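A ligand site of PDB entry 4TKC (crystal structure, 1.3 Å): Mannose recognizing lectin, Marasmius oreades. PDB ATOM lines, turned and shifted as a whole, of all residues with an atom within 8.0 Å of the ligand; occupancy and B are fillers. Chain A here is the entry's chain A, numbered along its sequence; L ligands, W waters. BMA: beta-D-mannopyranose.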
ATOM      1  N   LYS A  62      24.833  18.345  13.352  1.00  0.00           N
ATOM      2  CA  LYS A  62      25.016  17.364  14.399  1.00  0.00           C
ATOM      3  C   LYS A  62      25.543  16.081  13.762  1.00  0.00           C
ATOM      4  O   LYS A  62      24.891  15.514  12.864  1.00  0.00           O
ATOM      5  CB  LYS A  62      23.673  17.125  15.120  1.00  0.00           C
ATOM      6  CG  LYS A  62      23.776  16.144  16.296  1.00  0.00           C
ATOM      7  CD  LYS A  62      22.543  16.262  17.179  1.00  0.00           C
ATOM      8  CE  LYS A  62      22.690  15.560  18.514  1.00  0.00           C
ATOM      9  NZ  LYS A  62      21.439  15.517  19.350  1.00  0.00           N
ATOM     10  N   GLN A  64      25.476  12.558  14.471  1.00  0.00           N
ATOM     11  CA  GLN A  64      24.553  11.816  15.337  1.00  0.00           C
ATOM     12  C   GLN A  64      25.040  10.433  15.716  1.00  0.00           C
ATOM     13  O   GLN A  64      25.795   9.774  14.956  1.00  0.00           O
ATOM     14  CB  GLN A  64      23.212  11.684  14.627  1.00  0.00           C
ATOM     15  CG  GLN A  64      22.588  13.015  14.275  1.00  0.00           C
ATOM     16  CD  GLN A  64      21.238  12.917  13.612  1.00  0.00           C
ATOM     17  OE1 GLN A  64      20.871  11.906  12.999  1.00  0.00           O
ATOM     18  NE2 GLN A  64      20.510  14.022  13.672  1.00  0.00           N
ATOM     19  N   THR A  65      24.459   9.922  16.798  1.00  0.00           N
ATOM     20  CA  THR A  65      24.768   8.569  17.229  1.00  0.00           C
ATOM     21  C   THR A  65      24.246   7.486  16.252  1.00  0.00           C
ATOM     22  O   THR A  65      24.681   6.338  16.353  1.00  0.00           O
ATOM     23  CB  THR A  65      24.189   8.278  18.591  1.00  0.00           C
ATOM     24  OG1 THR A  65      22.797   8.573  18.551  1.00  0.00           O
ATOM     25  CG2 THR A  65      24.839   9.151  19.690  1.00  0.00           C
ATOM     26  N   ASP A  66      23.375   7.848  15.297  1.00  0.00           N
ATOM     27  CA  ASP A  66      23.024   6.881  14.224  1.00  0.00           C
ATOM     28  C   ASP A  66      24.017   6.823  13.055  1.00  0.00           C
ATOM     29  O   ASP A  66      23.806   6.020  12.148  1.00  0.00           O
ATOM     30  CB  ASP A  66      21.563   7.067  13.745  1.00  0.00           C
ATOM     31  CG  ASP A  66      21.325   8.348  12.973  1.00  0.00           C
ATOM     32  OD1 ASP A  66      22.314   9.118  12.792  1.00  0.00           O
ATOM     33  OD2 ASP A  66      20.163   8.561  12.529  1.00  0.00           O
ATOM     34  N   GLY A  67      25.100   7.612  13.144  1.00  0.00           N
ATOM     35  CA  GLY A  67      26.111   7.642  12.076  1.00  0.00           C
ATOM     36  C   GLY A  67      25.836   8.720  11.061  1.00  0.00           C
ATOM     37  O   GLY A  67      26.649   8.912  10.156  1.00  0.00           O
ATOM     38  N   ASN A  68      24.634   9.255  11.034  1.00  0.00           N
ATOM     39  CA  ASN A  68      24.270  10.307  10.090  1.00  0.00           C
ATOM     40  C   ASN A  68      24.784  11.649  10.560  1.00  0.00           C
ATOM     41  O   ASN A  68      24.633  11.951  11.735  1.00  0.00           O
ATOM     42  CB  ASN A  68      22.753  10.350   9.812  1.00  0.00           C
ATOM     43  CG  ASN A  68      22.393  10.864   8.411  1.00  0.00           C
ATOM     44  OD1 ASN A  68      23.250  11.138   7.553  1.00  0.00           O
ATOM     45  ND2 ASN A  68      21.079  11.002   8.180  1.00  0.00           N
ATOM     46  N   CYS A  69      25.364  12.442   9.662  1.00  0.00           N
ATOM     47  CA  CYS A  69      25.749  13.815   9.929  1.00  0.00           C
ATOM     48  C   CYS A  69      24.770  14.764   9.270  1.00  0.00           C
ATOM     49  O   CYS A  69      24.566  14.705   8.058  1.00  0.00           O
ATOM     50  CB  CYS A  69      27.180  14.109   9.472  1.00  0.00           C
ATOM     51  SG  CYS A  69      27.737  15.756   9.942  1.00  0.00           S
ATOM     52  N   VAL A  70      24.075  15.585  10.087  1.00  0.00           N
ATOM     53  CA  VAL A  70      22.850  16.226   9.642  1.00  0.00           C
ATOM     54  C   VAL A  70      22.901  17.695   9.966  1.00  0.00           C
ATOM     55  O   VAL A  70      23.158  18.059  11.114  1.00  0.00           O
ATOM     56  CB  VAL A  70      21.590  15.559  10.228  1.00  0.00           C
ATOM     57  CG1 VAL A  70      20.356  16.065   9.511  1.00  0.00           C
ATOM     58  CG2 VAL A  70      21.660  14.038  10.107  1.00  0.00           C
ATOM     59  N   GLY A  71      22.510  18.517   8.999  1.00  0.00           N
ATOM     60  CA  GLY A  71      22.273  19.939   9.239  1.00  0.00           C
ATOM     61  C   GLY A  71      20.759  20.155   9.382  1.00  0.00           C
ATOM     62  O   GLY A  71      19.946  19.501   8.717  1.00  0.00           O
ATOM     63  N   TYR A  72      20.394  20.938  10.428  1.00  0.00           N
ATOM     64  CA  TYR A  72      18.981  21.208  10.763  1.00  0.00           C
ATOM     65  C   TYR A  72      18.684  22.689  10.740  1.00  0.00           C
ATOM     66  O   TYR A  72      19.519  23.499  11.129  1.00  0.00           O
ATOM     67  CB  TYR A  72      18.624  20.632  12.145  1.00  0.00           C
ATOM     68  CG  TYR A  72      18.588  19.129  12.250  1.00  0.00           C
ATOM     69  CD1 TYR A  72      17.467  18.425  11.884  1.00  0.00           C
ATOM     70  CD2 TYR A  72      19.672  18.403  12.745  1.00  0.00           C
ATOM     71  CE1 TYR A  72      17.423  17.039  11.949  1.00  0.00           C
ATOM     72  CE2 TYR A  72      19.638  17.027  12.837  1.00  0.00           C
ATOM     73  CZ  TYR A  72      18.505  16.337  12.464  1.00  0.00           C
ATOM     74  OH  TYR A  72      18.471  14.987  12.474  1.00  0.00           O
ATOM     75  N   GLY A  76      14.033  22.103  13.450  1.00  0.00           N
ATOM     76  CA  GLY A  76      14.394  20.695  13.497  1.00  0.00           C
ATOM     77  C   GLY A  76      14.201  19.943  12.188  1.00  0.00           C
ATOM     78  O   GLY A  76      14.219  18.710  12.166  1.00  0.00           O
ATOM     79  N   THR A  77      13.952  20.679  11.101  1.00  0.00           N
ATOM     80  CA  THR A  77      13.886  20.077   9.749  1.00  0.00           C
ATOM     81  C   THR A  77      15.293  19.891   9.187  1.00  0.00           C
ATOM     82  O   THR A  77      16.103  20.797   9.271  1.00  0.00           O
ATOM     83  CB  THR A  77      13.054  20.971   8.787  1.00  0.00           C
ATOM     84  OG1 THR A  77      11.763  21.200   9.369  1.00  0.00           O
ATOM     85  CG2 THR A  77      12.896  20.333   7.415  1.00  0.00           C
ATOM     86  N   ALA A  78      15.565  18.695   8.670  1.00  0.00           N
ATOM     87  CA  ALA A  78      16.878  18.418   8.048  1.00  0.00           C
ATOM     88  C   ALA A  78      17.082  19.189   6.736  1.00  0.00           C
ATOM     89  O   ALA A  78      16.175  19.231   5.922  1.00  0.00           O
ATOM     90  CB  ALA A  78      17.051  16.921   7.830  1.00  0.00           C
ATOM     91  N   VAL A  79      18.170  19.955   6.672  1.00  0.00           N
ATOM     92  CA  VAL A  79      18.497  20.683   5.449  1.00  0.00           C
ATOM     93  C   VAL A  79      19.715  20.112   4.722  1.00  0.00           C
ATOM     94  O   VAL A  79      20.030  20.538   3.607  1.00  0.00           O
ATOM     95  CB  VAL A  79      18.716  22.189   5.674  1.00  0.00           C
ATOM     96  CG1 VAL A  79      17.467  22.834   6.298  1.00  0.00           C
ATOM     97  CG2 VAL A  79      19.949  22.445   6.541  1.00  0.00           C
ATOM     98  N   TRP A  80      20.394  19.156   5.332  1.00  0.00           N
ATOM     99  CA  TRP A  80      21.604  18.512   4.721  1.00  0.00           C
ATOM    100  C   TRP A  80      21.860  17.213   5.458  1.00  0.00           C
ATOM    101  O   TRP A  80      21.646  17.158   6.675  1.00  0.00           O
ATOM    102  CB  TRP A  80      22.832  19.387   4.908  1.00  0.00           C
ATOM    103  CG  TRP A  80      24.130  18.676   4.552  1.00  0.00           C
ATOM    104  CD1 TRP A  80      24.494  18.131   3.333  1.00  0.00           C
ATOM    105  CD2 TRP A  80      25.251  18.494   5.423  1.00  0.00           C
ATOM    106  NE1 TRP A  80      25.747  17.568   3.434  1.00  0.00           N
ATOM    107  CE2 TRP A  80      26.255  17.812   4.690  1.00  0.00           C
ATOM    108  CE3 TRP A  80      25.508  18.873   6.773  1.00  0.00           C
ATOM    109  CZ2 TRP A  80      27.477  17.468   5.246  1.00  0.00           C
ATOM    110  CZ3 TRP A  80      26.746  18.590   7.308  1.00  0.00           C
ATOM    111  CH2 TRP A  80      27.737  17.896   6.525  1.00  0.00           C
ATOM    112  N   HIS A  81      22.213  16.135   4.789  1.00  0.00           N
ATOM    113  CA  HIS A  81      22.667  14.958   5.500  1.00  0.00           C
ATOM    114  C   HIS A  81      23.619  14.143   4.643  1.00  0.00           C
ATOM    115  O   HIS A  81      23.543  14.158   3.408  1.00  0.00           O
ATOM    116  CB  HIS A  81      21.488  14.128   6.032  1.00  0.00           C
ATOM    117  CG  HIS A  81      20.552  13.662   4.967  1.00  0.00           C
ATOM    118  ND1 HIS A  81      20.538  12.356   4.509  1.00  0.00           N
ATOM    119  CD2 HIS A  81      19.609  14.320   4.258  1.00  0.00           C
ATOM    120  CE1 HIS A  81      19.620  12.229   3.573  1.00  0.00           C
ATOM    121  NE2 HIS A  81      19.066  13.419   3.374  1.00  0.00           N
ATOM    122  N   THR A  82      24.609  13.571   5.299  1.00  0.00           N
ATOM    123  CA  THR A  82      25.610  12.707   4.664  1.00  0.00           C
ATOM    124  C   THR A  82      25.101  11.296   4.349  1.00  0.00           C
ATOM    125  O   THR A  82      25.699  10.589   3.526  1.00  0.00           O
ATOM    126  CB  THR A  82      26.878  12.607   5.521  1.00  0.00           C
ATOM    127  OG1 THR A  82      26.488  12.101   6.822  1.00  0.00           O
ATOM    128  CG2 THR A  82      27.476  13.991   5.725  1.00  0.00           C
ATOM    129  N   ALA A  83      23.948  10.921   4.889  1.00  0.00           N
ATOM    130  CA  ALA A  83      23.369   9.589   4.643  1.00  0.00           C
ATOM    131  C   ALA A  83      24.344   8.444   4.916  1.00  0.00           C
ATOM    132  O   ALA A  83      24.396   7.452   4.208  1.00  0.00           O
ATOM    133  CB  ALA A  83      22.746   9.496   3.244  1.00  0.00           C
ATOM    134  N   THR A  84      25.033   8.586   6.038  1.00  0.00           N
ATOM    135  CA  THR A  84      26.062   7.684   6.469  1.00  0.00           C
ATOM    136  C   THR A  84      25.645   6.735   7.603  1.00  0.00           C
ATOM    137  O   THR A  84      26.507   6.002   8.134  1.00  0.00           O
ATOM    138  CB  THR A  84      27.317   8.466   6.860  1.00  0.00           C
ATOM    139  OG1 THR A  84      26.986   9.617   7.622  1.00  0.00           O
ATOM    140  CG2 THR A  84      28.007   8.931   5.626  1.00  0.00           C
ATOM    141  N   ASN A  85      24.333   6.693   7.901  1.00  0.00           N
ATOM    142  CA  ASN A  85      23.731   5.889   8.970  1.00  0.00           C
ATOM    143  C   ASN A  85      24.317   4.495   8.916  1.00  0.00           C
ATOM    144  O   ASN A  85      24.323   3.867   7.862  1.00  0.00           O
ATOM    145  CB  ASN A  85      22.207   5.693   8.771  1.00  0.00           C
ATOM    146  CG  ASN A  85      21.422   6.966   8.726  1.00  0.00           C
ATOM    147  OD1 ASN A  85      20.541   7.204   9.594  1.00  0.00           O
ATOM    148  ND2 ASN A  85      21.653   7.760   7.718  1.00  0.00           N
HETATM  149  C1  BMA L   1      17.418   9.967   9.380  1.00  0.00           C
HETATM  150  C2  BMA L   1      18.031  10.229  10.755  1.00  0.00           C
HETATM  151  C3  BMA L   1      17.423  11.515  11.272  1.00  0.00           C
HETATM  152  C4  BMA L   1      17.607  12.666  10.267  1.00  0.00           C
HETATM  153  C5  BMA L   1      17.087  12.287   8.874  1.00  0.00           C
HETATM  154  C6  BMA L   1      17.303  13.432   7.887  1.00  0.00           C
HETATM  155  O1  BMA L   1      17.986   8.732   8.939  1.00  0.00           O
HETATM  156  O2  BMA L   1      19.458  10.271  10.685  1.00  0.00           O
HETATM  157  O3  BMA L   1      18.022  11.809  12.545  1.00  0.00           O
HETATM  158  O4  BMA L   1      16.925  13.838  10.703  1.00  0.00           O
HETATM  159  O5  BMA L   1      17.741  11.065   8.498  1.00  0.00           O
HETATM  160  O6  BMA L   1      17.803  13.021   6.608  1.00  0.00           O
HETATM  161  O   HOH W   1      17.766  10.607   5.947  1.00  0.00           O
HETATM  162  O   HOH W   2      18.468  10.148  14.884  1.00  0.00           O
HETATM  163  O   HOH W   3      14.701  14.072  11.803  1.00  0.00           O
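The side-chain carboxylate of Asp 66 sits at hydrogen-bond distance from an oxygen (O2) of the ligand, at 2.6 Å.
O4 of the ligand lies within hydrogen-bond range of OH of Tyr 72, 2.6 Å away.
The side-chain amide oxygen (OE1) of Gln 64 lies within hydrogen-bond range of an oxygen (O3) of the ligand, at 2.9 Å.
OD1 of Asn 85 is in hydrogen-bond range of O1 of the ligand.
ND2 of Asn 68 is in hydrogen-bond range of O2 of the ligand (3.1 Å).
A ring nitrogen (NE2) of His 81 sits close to an oxygen (O6) of the ligand (3.5 Å).
The side-chain amide oxygen (OE1) of Gln 64 lies close to the side-chain carboxylate (OD1) of Asp 66, 3.1 Å away.
OD2 of Asp 66 lies close to OD1 of Asn 85 (3.3 Å).
OD1 of Asp 66 is in hydrogen-bond range of N of Asn 68 (2.9 Å).
The side-chain hydroxyl (OH) of Tyr 72 sits at hydrogen-bond distance from the side-chain amide nitrogen (NE2) of Gln 64 (2.6 Å).
ND2 of Asn 85 lies close to ND2 of Asn 68, 3.3 Å away.
The side-chain amide oxygen (OD1) of Asn 68 sits at hydrogen-bond distance from the backbone NH (N) of Ala 83 (2.8 Å).
OD1 of Asn 68 sits at hydrogen-bond distance from OG1 of Thr 82, 3.5 Å away.
N of Thr 84 sits at hydrogen-bond distance from OD1 of Asn 68 (3.5 Å).
Merely in contact with the ligand: Ala 78 (3.5 Å).
Within 4 Å of the ligand: Gln 64, Asp 66, Asn 68, Tyr 72, Ala 78, His 81 and Asn 85.
Along chain A the residues within 4 Å of the ligand span positions 64 to 85.
Water W2 bridges an oxygen (O3) of the ligand and the side-chain carboxylate (OD2) of Asp 66.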
